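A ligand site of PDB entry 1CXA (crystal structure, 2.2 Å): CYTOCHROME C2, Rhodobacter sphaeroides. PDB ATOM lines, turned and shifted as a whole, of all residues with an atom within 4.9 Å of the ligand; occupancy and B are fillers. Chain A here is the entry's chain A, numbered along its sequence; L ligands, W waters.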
ATOM      1  N   GLN A  14     -15.550   8.091  21.686  1.00  0.00           N
ATOM      2  CA  GLN A  14     -15.117   8.259  23.083  1.00  0.00           C
ATOM      3  C   GLN A  14     -14.251   7.108  23.580  1.00  0.00           C
ATOM      4  O   GLN A  14     -13.723   7.143  24.677  1.00  0.00           O
ATOM      5  CB  GLN A  14     -16.304   8.330  24.005  1.00  0.00           C
ATOM      6  CG  GLN A  14     -17.198   9.524  23.736  1.00  0.00           C
ATOM      7  CD  GLN A  14     -18.525   9.453  24.471  1.00  0.00           C
ATOM      8  OE1 GLN A  14     -19.588   9.216  23.864  1.00  0.00           O
ATOM      9  NE2 GLN A  14     -18.501   9.661  25.799  1.00  0.00           N
ATOM     10  N   CYS A  15     -14.540   5.914  23.075  1.00  0.00           N
ATOM     11  CA  CYS A  15     -13.846   4.717  23.484  1.00  0.00           C
ATOM     12  C   CYS A  15     -12.557   4.461  22.758  1.00  0.00           C
ATOM     13  O   CYS A  15     -11.782   3.678  23.257  1.00  0.00           O
ATOM     14  CB  CYS A  15     -14.749   3.524  23.239  1.00  0.00           C
ATOM     15  SG  CYS A  15     -16.453   3.976  23.544  1.00  0.00           S
ATOM     16  N   THR A  17      -9.960   6.058  22.480  1.00  0.00           N
ATOM     17  CA  THR A  17      -8.730   6.509  23.083  1.00  0.00           C
ATOM     18  C   THR A  17      -8.083   5.344  23.766  1.00  0.00           C
ATOM     19  O   THR A  17      -6.860   5.211  23.772  1.00  0.00           O
ATOM     20  CB  THR A  17      -9.027   7.516  24.153  1.00  0.00           C
ATOM     21  OG1 THR A  17      -9.756   8.535  23.502  1.00  0.00           O
ATOM     22  CG2 THR A  17      -7.728   8.067  24.730  1.00  0.00           C
ATOM     23  N   CYS A  18      -8.912   4.371  24.206  1.00  0.00           N
ATOM     24  CA  CYS A  18      -8.368   3.223  24.887  1.00  0.00           C
ATOM     25  C   CYS A  18      -8.694   1.881  24.248  1.00  0.00           C
ATOM     26  O   CYS A  18      -8.120   0.872  24.634  1.00  0.00           O
ATOM     27  CB  CYS A  18      -8.856   3.212  26.330  1.00  0.00           C
ATOM     28  SG  CYS A  18      -8.444   4.669  27.305  1.00  0.00           S
ATOM     29  N   HIS A  19      -9.726   1.784  23.395  1.00  0.00           N
ATOM     30  CA  HIS A  19     -10.016   0.482  22.832  1.00  0.00           C
ATOM     31  C   HIS A  19      -9.870   0.520  21.323  1.00  0.00           C
ATOM     32  O   HIS A  19     -10.300   1.460  20.687  1.00  0.00           O
ATOM     33  CB  HIS A  19     -11.442   0.063  23.128  1.00  0.00           C
ATOM     34  CG  HIS A  19     -11.700  -0.139  24.621  1.00  0.00           C
ATOM     35  ND1 HIS A  19     -11.464  -1.364  25.182  1.00  0.00           N
ATOM     36  CD2 HIS A  19     -12.284   0.746  25.556  1.00  0.00           C
ATOM     37  CE1 HIS A  19     -11.928  -1.235  26.456  1.00  0.00           C
ATOM     38  NE2 HIS A  19     -12.394  -0.051  26.719  1.00  0.00           N
ATOM     39  N   THR A  36      -4.631   0.492  26.006  1.00  0.00           N
ATOM     40  CA  THR A  36      -5.042   0.597  27.385  1.00  0.00           C
ATOM     41  C   THR A  36      -6.160  -0.383  27.726  1.00  0.00           C
ATOM     42  O   THR A  36      -6.151  -1.025  28.775  1.00  0.00           O
ATOM     43  CB  THR A  36      -5.543   2.003  27.654  1.00  0.00           C
ATOM     44  OG1 THR A  36      -4.474   2.836  27.250  1.00  0.00           O
ATOM     45  CG2 THR A  36      -5.945   2.228  29.115  1.00  0.00           C
ATOM     46  N   GLY A  37      -7.203  -0.430  26.909  1.00  0.00           N
ATOM     47  CA  GLY A  37      -8.304  -1.332  27.201  1.00  0.00           C
ATOM     48  C   GLY A  37      -8.209  -2.534  26.310  1.00  0.00           C
ATOM     49  O   GLY A  37      -7.558  -2.415  25.276  1.00  0.00           O
ATOM     50  N   PRO A  38      -9.137  -3.492  26.437  1.00  0.00           N
ATOM     51  CA  PRO A  38      -9.081  -4.707  25.642  1.00  0.00           C
ATOM     52  C   PRO A  38      -9.653  -4.521  24.236  1.00  0.00           C
ATOM     53  O   PRO A  38     -10.423  -3.614  23.994  1.00  0.00           O
ATOM     54  CB  PRO A  38      -9.916  -5.717  26.430  1.00  0.00           C
ATOM     55  CG  PRO A  38     -10.548  -5.003  27.602  1.00  0.00           C
ATOM     56  CD  PRO A  38      -9.841  -3.674  27.708  1.00  0.00           C
ATOM     57  N   LEU A  40     -12.263  -4.629  21.665  1.00  0.00           N
ATOM     58  CA  LEU A  40     -13.689  -4.872  21.906  1.00  0.00           C
ATOM     59  C   LEU A  40     -14.354  -5.752  20.867  1.00  0.00           C
ATOM     60  O   LEU A  40     -15.581  -5.886  20.817  1.00  0.00           O
ATOM     61  CB  LEU A  40     -14.383  -3.514  21.953  1.00  0.00           C
ATOM     62  CG  LEU A  40     -14.818  -2.992  23.294  1.00  0.00           C
ATOM     63  CD1 LEU A  40     -14.049  -3.637  24.405  1.00  0.00           C
ATOM     64  CD2 LEU A  40     -14.693  -1.496  23.298  1.00  0.00           C
ATOM     65  N   VAL A  43     -16.750  -8.779  21.898  1.00  0.00           N
ATOM     66  CA  VAL A  43     -17.118  -8.576  23.294  1.00  0.00           C
ATOM     67  C   VAL A  43     -18.560  -8.964  23.536  1.00  0.00           C
ATOM     68  O   VAL A  43     -18.959  -9.178  24.686  1.00  0.00           O
ATOM     69  CB  VAL A  43     -16.947  -7.095  23.670  1.00  0.00           C
ATOM     70  CG1 VAL A  43     -17.916  -6.242  22.875  1.00  0.00           C
ATOM     71  CG2 VAL A  43     -17.178  -6.859  25.146  1.00  0.00           C
ATOM     72  N   ARG A  46     -19.348 -11.920  25.545  1.00  0.00           N
ATOM     73  CA  ARG A  46     -18.104 -12.514  26.009  1.00  0.00           C
ATOM     74  C   ARG A  46     -17.998 -12.481  27.525  1.00  0.00           C
ATOM     75  O   ARG A  46     -18.635 -11.676  28.211  1.00  0.00           O
ATOM     76  CB  ARG A  46     -16.989 -11.726  25.389  1.00  0.00           C
ATOM     77  CG  ARG A  46     -15.639 -12.424  25.433  1.00  0.00           C
ATOM     78  CD  ARG A  46     -14.569 -11.381  25.683  1.00  0.00           C
ATOM     79  NE  ARG A  46     -14.014 -10.877  24.450  1.00  0.00           N
ATOM     80  CZ  ARG A  46     -13.790  -9.580  24.341  1.00  0.00           C
ATOM     81  NH1 ARG A  46     -13.994  -8.821  25.385  1.00  0.00           N
ATOM     82  NH2 ARG A  46     -13.292  -9.095  23.236  1.00  0.00           N
ATOM     83  N   THR A  47     -17.268 -13.438  28.109  1.00  0.00           N
ATOM     84  CA  THR A  47     -17.166 -13.448  29.541  1.00  0.00           C
ATOM     85  C   THR A  47     -16.228 -12.370  29.974  1.00  0.00           C
ATOM     86  O   THR A  47     -15.145 -12.170  29.412  1.00  0.00           O
ATOM     87  CB  THR A  47     -16.675 -14.818  30.052  1.00  0.00           C
ATOM     88  OG1 THR A  47     -17.761 -15.702  29.886  1.00  0.00           O
ATOM     89  CG2 THR A  47     -16.268 -14.827  31.521  1.00  0.00           C
ATOM     90  N   ALA A  48     -16.744 -11.527  30.827  1.00  0.00           N
ATOM     91  CA  ALA A  48     -15.987 -10.409  31.328  1.00  0.00           C
ATOM     92  C   ALA A  48     -14.559 -10.735  31.745  1.00  0.00           C
ATOM     93  O   ALA A  48     -14.297 -11.806  32.263  1.00  0.00           O
ATOM     94  CB  ALA A  48     -16.732  -9.906  32.542  1.00  0.00           C
ATOM     95  N   GLY A  49     -13.573  -9.953  31.328  1.00  0.00           N
ATOM     96  CA  GLY A  49     -12.222 -10.193  31.797  1.00  0.00           C
ATOM     97  C   GLY A  49     -11.552 -11.411  31.195  1.00  0.00           C
ATOM     98  O   GLY A  49     -10.538 -11.898  31.705  1.00  0.00           O
ATOM     99  N   GLN A  51     -10.653 -11.392  27.522  1.00  0.00           N
ATOM    100  CA  GLN A  51     -10.067 -11.244  26.182  1.00  0.00           C
ATOM    101  C   GLN A  51      -8.647 -11.816  26.134  1.00  0.00           C
ATOM    102  O   GLN A  51      -7.676 -11.188  26.553  1.00  0.00           O
ATOM    103  CB  GLN A  51     -10.070  -9.795  25.750  1.00  0.00           C
ATOM    104  CG  GLN A  51     -10.271  -9.644  24.254  1.00  0.00           C
ATOM    105  CD  GLN A  51      -8.970  -9.796  23.467  1.00  0.00           C
ATOM    106  OE1 GLN A  51      -7.882  -9.419  23.904  1.00  0.00           O
ATOM    107  NE2 GLN A  51      -9.044 -10.365  22.280  1.00  0.00           N
ATOM    108  N   PHE A  54      -5.561  -9.422  26.208  1.00  0.00           N
ATOM    109  CA  PHE A  54      -5.421  -8.379  27.205  1.00  0.00           C
ATOM    110  C   PHE A  54      -4.688  -8.842  28.445  1.00  0.00           C
ATOM    111  O   PHE A  54      -5.208  -9.623  29.226  1.00  0.00           O
ATOM    112  CB  PHE A  54      -6.782  -7.800  27.574  1.00  0.00           C
ATOM    113  CG  PHE A  54      -6.647  -6.409  28.179  1.00  0.00           C
ATOM    114  CD1 PHE A  54      -5.997  -5.421  27.477  1.00  0.00           C
ATOM    115  CD2 PHE A  54      -7.121  -6.145  29.440  1.00  0.00           C
ATOM    116  CE1 PHE A  54      -5.832  -4.178  28.054  1.00  0.00           C
ATOM    117  CE2 PHE A  54      -6.940  -4.895  30.008  1.00  0.00           C
ATOM    118  CZ  PHE A  54      -6.298  -3.911  29.311  1.00  0.00           C
ATOM    119  N   GLY A  56      -4.034  -6.274  30.977  1.00  0.00           N
ATOM    120  CA  GLY A  56      -4.241  -5.332  32.080  1.00  0.00           C
ATOM    121  C   GLY A  56      -5.598  -5.362  32.810  1.00  0.00           C
ATOM    122  O   GLY A  56      -5.909  -4.413  33.540  1.00  0.00           O
ATOM    123  N   TYR A  57      -6.241  -6.531  32.897  1.00  0.00           N
ATOM    124  CA  TYR A  57      -7.526  -6.597  33.557  1.00  0.00           C
ATOM    125  C   TYR A  57      -7.351  -6.475  35.044  1.00  0.00           C
ATOM    126  O   TYR A  57      -6.399  -7.014  35.603  1.00  0.00           O
ATOM    127  CB  TYR A  57      -8.209  -7.930  33.311  1.00  0.00           C
ATOM    128  CG  TYR A  57      -8.880  -8.027  31.967  1.00  0.00           C
ATOM    129  CD1 TYR A  57      -9.962  -7.239  31.680  1.00  0.00           C
ATOM    130  CD2 TYR A  57      -8.485  -8.991  31.068  1.00  0.00           C
ATOM    131  CE1 TYR A  57     -10.657  -7.428  30.494  1.00  0.00           C
ATOM    132  CE2 TYR A  57      -9.182  -9.194  29.891  1.00  0.00           C
ATOM    133  CZ  TYR A  57     -10.272  -8.410  29.608  1.00  0.00           C
ATOM    134  OH  TYR A  57     -10.991  -8.617  28.433  1.00  0.00           O
ATOM    135  N   GLY A  58      -8.292  -5.824  35.718  1.00  0.00           N
ATOM    136  CA  GLY A  58      -8.212  -5.716  37.151  1.00  0.00           C
ATOM    137  C   GLY A  58      -8.775  -6.985  37.770  1.00  0.00           C
ATOM    138  O   GLY A  58      -9.245  -7.875  37.070  1.00  0.00           O
ATOM    139  N   MET A  61     -12.612  -7.285  37.555  1.00  0.00           N
ATOM    140  CA  MET A  61     -13.132  -7.715  36.255  1.00  0.00           C
ATOM    141  C   MET A  61     -12.931  -9.218  36.051  1.00  0.00           C
ATOM    142  O   MET A  61     -13.800  -9.924  35.542  1.00  0.00           O
ATOM    143  CB  MET A  61     -12.405  -6.929  35.146  1.00  0.00           C
ATOM    144  CG  MET A  61     -12.900  -7.160  33.721  1.00  0.00           C
ATOM    145  SD  MET A  61     -14.636  -6.724  33.524  1.00  0.00           S
ATOM    146  CE  MET A  61     -14.517  -4.989  33.349  1.00  0.00           C
ATOM    147  N   TRP A  71     -20.952 -10.288  28.662  1.00  0.00           N
ATOM    148  CA  TRP A  71     -21.598  -9.018  28.306  1.00  0.00           C
ATOM    149  C   TRP A  71     -22.862  -9.033  27.455  1.00  0.00           C
ATOM    150  O   TRP A  71     -22.921  -9.622  26.375  1.00  0.00           O
ATOM    151  CB  TRP A  71     -20.532  -8.150  27.606  1.00  0.00           C
ATOM    152  CG  TRP A  71     -19.416  -7.763  28.557  1.00  0.00           C
ATOM    153  CD1 TRP A  71     -18.148  -8.263  28.384  1.00  0.00           C
ATOM    154  CD2 TRP A  71     -19.522  -6.911  29.629  1.00  0.00           C
ATOM    155  NE1 TRP A  71     -17.434  -7.731  29.356  1.00  0.00           N
ATOM    156  CE2 TRP A  71     -18.224  -6.917  30.119  1.00  0.00           C
ATOM    157  CE3 TRP A  71     -20.495  -6.187  30.273  1.00  0.00           C
ATOM    158  CZ2 TRP A  71     -17.879  -6.218  31.258  1.00  0.00           C
ATOM    159  CZ3 TRP A  71     -20.129  -5.475  31.415  1.00  0.00           C
ATOM    160  CH2 TRP A  71     -18.826  -5.492  31.910  1.00  0.00           C
ATOM    161  N   PHE A  76     -23.662  -4.231  30.107  1.00  0.00           N
ATOM    162  CA  PHE A  76     -22.744  -3.321  29.406  1.00  0.00           C
ATOM    163  C   PHE A  76     -23.083  -1.861  29.636  1.00  0.00           C
ATOM    164  O   PHE A  76     -22.244  -1.162  30.150  1.00  0.00           O
ATOM    165  CB  PHE A  76     -22.779  -3.651  27.923  1.00  0.00           C
ATOM    166  CG  PHE A  76     -22.121  -2.602  27.076  1.00  0.00           C
ATOM    167  CD1 PHE A  76     -22.845  -1.493  26.683  1.00  0.00           C
ATOM    168  CD2 PHE A  76     -20.799  -2.744  26.721  1.00  0.00           C
ATOM    169  CE1 PHE A  76     -22.246  -0.503  25.930  1.00  0.00           C
ATOM    170  CE2 PHE A  76     -20.197  -1.747  25.980  1.00  0.00           C
ATOM    171  CZ  PHE A  76     -20.922  -0.630  25.590  1.00  0.00           C
ATOM    172  N   TYR A  79     -22.486  -1.046  33.490  1.00  0.00           N
ATOM    173  CA  TYR A  79     -21.081  -0.940  33.676  1.00  0.00           C
ATOM    174  C   TYR A  79     -20.510   0.388  33.205  1.00  0.00           C
ATOM    175  O   TYR A  79     -19.715   0.950  33.901  1.00  0.00           O
ATOM    176  CB  TYR A  79     -20.410  -2.084  32.948  1.00  0.00           C
ATOM    177  CG  TYR A  79     -18.882  -2.123  33.082  1.00  0.00           C
ATOM    178  CD1 TYR A  79     -18.220  -2.182  34.298  1.00  0.00           C
ATOM    179  CD2 TYR A  79     -18.161  -2.091  31.915  1.00  0.00           C
ATOM    180  CE1 TYR A  79     -16.833  -2.164  34.319  1.00  0.00           C
ATOM    181  CE2 TYR A  79     -16.796  -2.077  31.937  1.00  0.00           C
ATOM    182  CZ  TYR A  79     -16.136  -2.104  33.127  1.00  0.00           C
ATOM    183  OH  TYR A  79     -14.756  -1.922  33.094  1.00  0.00           O
ATOM    184  N   VAL A  80     -20.487   0.666  31.887  1.00  0.00           N
ATOM    185  CA  VAL A  80     -19.935   1.925  31.444  1.00  0.00           C
ATOM    186  C   VAL A  80     -20.511   3.120  32.164  1.00  0.00           C
ATOM    187  O   VAL A  80     -19.872   4.152  32.221  1.00  0.00           O
ATOM    188  CB  VAL A  80     -20.081   2.126  29.929  1.00  0.00           C
ATOM    189  CG1 VAL A  80     -19.456   0.959  29.186  1.00  0.00           C
ATOM    190  CG2 VAL A  80     -21.547   2.231  29.529  1.00  0.00           C
ATOM    191  N   LEU A  87     -18.865  -3.061  39.531  1.00  0.00           N
ATOM    192  CA  LEU A  87     -18.016  -4.159  39.921  1.00  0.00           C
ATOM    193  C   LEU A  87     -18.252  -4.498  41.357  1.00  0.00           C
ATOM    194  O   LEU A  87     -18.136  -5.639  41.775  1.00  0.00           O
ATOM    195  CB  LEU A  87     -16.564  -3.799  39.724  1.00  0.00           C
ATOM    196  CG  LEU A  87     -16.064  -3.898  38.314  1.00  0.00           C
ATOM    197  CD1 LEU A  87     -14.619  -3.399  38.202  1.00  0.00           C
ATOM    198  CD2 LEU A  87     -16.196  -5.332  37.865  1.00  0.00           C
ATOM    199  N   GLY A  98     -11.584  -1.464  39.887  1.00  0.00           N
ATOM    200  CA  GLY A  98     -11.403  -1.660  38.480  1.00  0.00           C
ATOM    201  C   GLY A  98     -10.282  -0.814  37.935  1.00  0.00           C
ATOM    202  O   GLY A  98      -9.925   0.183  38.520  1.00  0.00           O
ATOM    203  N   LYS A  99      -9.918  -1.016  36.691  1.00  0.00           N
ATOM    204  CA  LYS A  99      -8.874  -0.200  36.161  1.00  0.00           C
ATOM    205  C   LYS A  99      -9.416   1.034  35.432  1.00  0.00           C
ATOM    206  O   LYS A  99      -8.699   1.811  34.843  1.00  0.00           O
ATOM    207  CB  LYS A  99      -7.996  -1.045  35.270  1.00  0.00           C
ATOM    208  CG  LYS A  99      -7.590  -2.299  36.020  1.00  0.00           C
ATOM    209  CD  LYS A  99      -6.074  -2.407  36.104  1.00  0.00           C
ATOM    210  N   MET A 100     -10.719   1.192  35.337  1.00  0.00           N
ATOM    211  CA  MET A 100     -11.234   2.392  34.727  1.00  0.00           C
ATOM    212  C   MET A 100     -12.467   2.783  35.520  1.00  0.00           C
ATOM    213  O   MET A 100     -13.473   2.098  35.537  1.00  0.00           O
ATOM    214  CB  MET A 100     -11.516   2.208  33.241  1.00  0.00           C
ATOM    215  CG  MET A 100     -11.300   3.498  32.408  1.00  0.00           C
ATOM    216  SD  MET A 100     -12.805   4.484  32.456  1.00  0.00           S
ATOM    217  CE  MET A 100     -12.787   5.496  31.002  1.00  0.00           C
ATOM    218  N   LEU A 104     -19.750   7.081  32.281  1.00  0.00           N
ATOM    219  CA  LEU A 104     -20.223   7.618  31.044  1.00  0.00           C
ATOM    220  C   LEU A 104     -21.161   8.752  31.350  1.00  0.00           C
ATOM    221  O   LEU A 104     -22.180   8.487  31.985  1.00  0.00           O
ATOM    222  CB  LEU A 104     -20.998   6.576  30.246  1.00  0.00           C
ATOM    223  CG  LEU A 104     -21.104   6.837  28.736  1.00  0.00           C
ATOM    224  CD1 LEU A 104     -19.761   6.642  28.067  1.00  0.00           C
ATOM    225  CD2 LEU A 104     -22.138   5.956  28.082  1.00  0.00           C
ATOM    226  N   ILE A 113     -23.807   2.751  21.370  1.00  0.00           N
ATOM    227  CA  ILE A 113     -22.610   2.007  21.068  1.00  0.00           C
ATOM    228  C   ILE A 113     -22.897   0.529  21.063  1.00  0.00           C
ATOM    229  O   ILE A 113     -22.350  -0.200  20.262  1.00  0.00           O
ATOM    230  CB  ILE A 113     -21.530   2.353  22.079  1.00  0.00           C
ATOM    231  CG1 ILE A 113     -21.150   3.822  21.959  1.00  0.00           C
ATOM    232  CG2 ILE A 113     -20.323   1.438  21.877  1.00  0.00           C
ATOM    233  CD1 ILE A 113     -20.394   4.319  23.189  1.00  0.00           C
HETATM  234 FE1  LIG L   1     -13.350   0.543  28.369  1.00  0.00          FE
HETATM  235  C1  LIG L   1     -12.847  -2.478  29.907  1.00  0.00           C
HETATM  236  C2  LIG L   1     -16.257  -0.590  27.122  1.00  0.00           C
HETATM  237  C3  LIG L   1     -13.894   3.597  27.003  1.00  0.00           C
HETATM  238  C4  LIG L   1     -10.337   1.606  29.538  1.00  0.00           C
HETATM  239  N1  LIG L   1     -14.293  -1.172  28.442  1.00  0.00           N
HETATM  240  C5  LIG L   1     -13.963  -2.337  29.133  1.00  0.00           C
HETATM  241  C6  LIG L   1     -14.966  -3.366  28.954  1.00  0.00           C
HETATM  242  C7  LIG L   1     -15.953  -2.817  28.199  1.00  0.00           C
HETATM  243  C8  LIG L   1     -15.515  -1.481  27.867  1.00  0.00           C
HETATM  244  C9  LIG L   1     -17.312  -3.455  27.942  1.00  0.00           C
HETATM  245  C10 LIG L   1     -14.878  -4.829  29.400  1.00  0.00           C
HETATM  246  C11 LIG L   1     -14.499  -5.677  28.216  1.00  0.00           C
HETATM  247  C12 LIG L   1     -13.926  -6.984  28.632  1.00  0.00           C
HETATM  248  O1  LIG L   1     -13.099  -7.485  27.894  1.00  0.00           O
HETATM  249  O2  LIG L   1     -14.555  -7.639  29.435  1.00  0.00           O
HETATM  250  N2  LIG L   1     -14.722   1.330  27.235  1.00  0.00           N
HETATM  251  C13 LIG L   1     -15.887   0.721  26.825  1.00  0.00           C
HETATM  252  C14 LIG L   1     -16.724   1.607  26.054  1.00  0.00           C
HETATM  253  C15 LIG L   1     -16.065   2.817  25.982  1.00  0.00           C
HETATM  254  C16 LIG L   1     -14.830   2.616  26.735  1.00  0.00           C
HETATM  255  C17 LIG L   1     -18.035   1.166  25.396  1.00  0.00           C
HETATM  256  C18 LIG L   1     -16.523   4.000  25.355  1.00  0.00           C
HETATM  257  C19 LIG L   1     -17.796   4.619  25.716  1.00  0.00           C
HETATM  258  N3  LIG L   1     -12.351   2.229  28.337  1.00  0.00           N
HETATM  259  C20 LIG L   1     -12.738   3.432  27.744  1.00  0.00           C
HETATM  260  C21 LIG L   1     -11.721   4.452  27.923  1.00  0.00           C
HETATM  261  C22 LIG L   1     -10.691   3.875  28.579  1.00  0.00           C
HETATM  262  C23 LIG L   1     -11.095   2.516  28.846  1.00  0.00           C
HETATM  263  C24 LIG L   1     -11.733   5.886  27.394  1.00  0.00           C
HETATM  264  C25 LIG L   1      -9.438   4.465  28.805  1.00  0.00           C
HETATM  265  C26 LIG L   1      -9.309   5.666  29.600  1.00  0.00           C
HETATM  266  N4  LIG L   1     -11.937  -0.252  29.461  1.00  0.00           N
HETATM  267  C27 LIG L   1     -10.726   0.321  29.843  1.00  0.00           C
HETATM  268  C28 LIG L   1      -9.962  -0.578  30.669  1.00  0.00           C
HETATM  269  C29 LIG L   1     -10.666  -1.692  30.837  1.00  0.00           C
HETATM  270  C30 LIG L   1     -11.880  -1.512  30.064  1.00  0.00           C
HETATM  271  C31 LIG L   1      -8.568  -0.318  31.217  1.00  0.00           C
HETATM  272  C32 LIG L   1     -10.379  -2.759  31.857  1.00  0.00           C
HETATM  273  C33 LIG L   1     -11.269  -2.621  33.076  1.00  0.00           C
HETATM  274  C34 LIG L   1     -10.675  -3.367  34.256  1.00  0.00           C
HETATM  275  O3  LIG L   1     -11.078  -3.116  35.393  1.00  0.00           O
HETATM  276  O4  LIG L   1      -9.990  -4.339  34.016  1.00  0.00           O
HETATM  277  O   HOH W   1     -13.200  -1.646  35.141  1.00  0.00           O
HETATM  278  O   HOH W   2     -11.117  -4.822  37.531  1.00  0.00           O
HETATM  279  O   HOH W   3     -13.720 -10.220  28.068  1.00  0.00           O
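Water W1 bridges OH of Tyr 79 (2.6 Å) and O3 of the ligand (2.6 Å). Water W2 bridges O3 of the ligand (2.7 Å) and N of Met 61 (2.9 Å).
The backbone carbonyl oxygen (O) of Pro 38 lies within hydrogen-bond range of a ring nitrogen (ND1) of His 19 (2.7 Å). O of Cys 18 lies within hydrogen-bond range of N of Gly 37 (2.8 Å). N of Leu 104 lies within hydrogen-bond range of O of Val 80, 2.9 Å away. N of Gln 51 sits at hydrogen-bond distance from OH of Tyr 57. The backbone NH (N) of Trp 71 is in hydrogen-bond range of the backbone carbonyl oxygen (O) of Arg 46.
Gln 14 touches the ligand. O of Thr 36 touches C31 of the ligand, 3.5 Å away. Gly 37 touches the ligand (CA to C28, 3.9 Å). CG of Pro 38 touches O1 of the ligand (3.6 Å). Ala 48 touches the ligand. CB of Met 61 touches O4 of the ligand, at 3.7 Å. Phe 76 touches the ligand. OH of Tyr 79 touches C33 of the ligand (3.6 Å). CA of Gly 98 touches O3 of the ligand, at 3.4 Å. Met 100 touches the ligand. Leu 104 touches the ligand. CD1 of Ile 113 touches C19 of the ligand, 3.6 Å away. Hydrophobic or aromatic side chains within 4 Å of the ligand: His 19, Pro 38, Tyr 57, Met 61, Trp 71, Phe 76, Tyr 79, Met 100, Leu 104 and Ile 113. Within 4 Å of the ligand: Gln 14, Cys 15, Cys 18, His 19, Thr 36, Gly 37, Pro 38, Arg 46, Ala 48, Gly 49, Tyr 57, Gly 58, Met 61, Trp 71, Phe 76, Tyr 79, Gly 98, Lys 99, Met 100, Leu 104 and Ile 113. The nearest printed residue that does not touch the ligand is Val 80 (4.1 Å).
An oxygen (O1) of the ligand sits at hydrogen-bond distance from the side-chain hydroxyl (OH) of Tyr 57 (2.5 Å). N of Gly 49 is in hydrogen-bond range of O2 of the ligand. An oxygen (O2) of the ligand lies within hydrogen-bond range of the indole nitrogen of Trp 71, 2.9 Å away. NE2 of His 19 is bound to FE1 of the ligand (2.0 Å). SG of Cys 18 is covalently linked to C25 of the ligand, at 1.8 Å. The side-chain sulfur (SG) of Cys 15 is covalently linked to a carbon (C18) of the ligand (1.8 Å). NH1 of Arg 46 is in salt-bridge range of O1 of the ligand, at 3.0 Å. The backbone NH (N) of Lys 99 is in hydrogen-bond range of an oxygen (O3) of the ligand (2.7 Å). N of Gly 58 is in hydrogen-bond range of O4 of the ligand.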
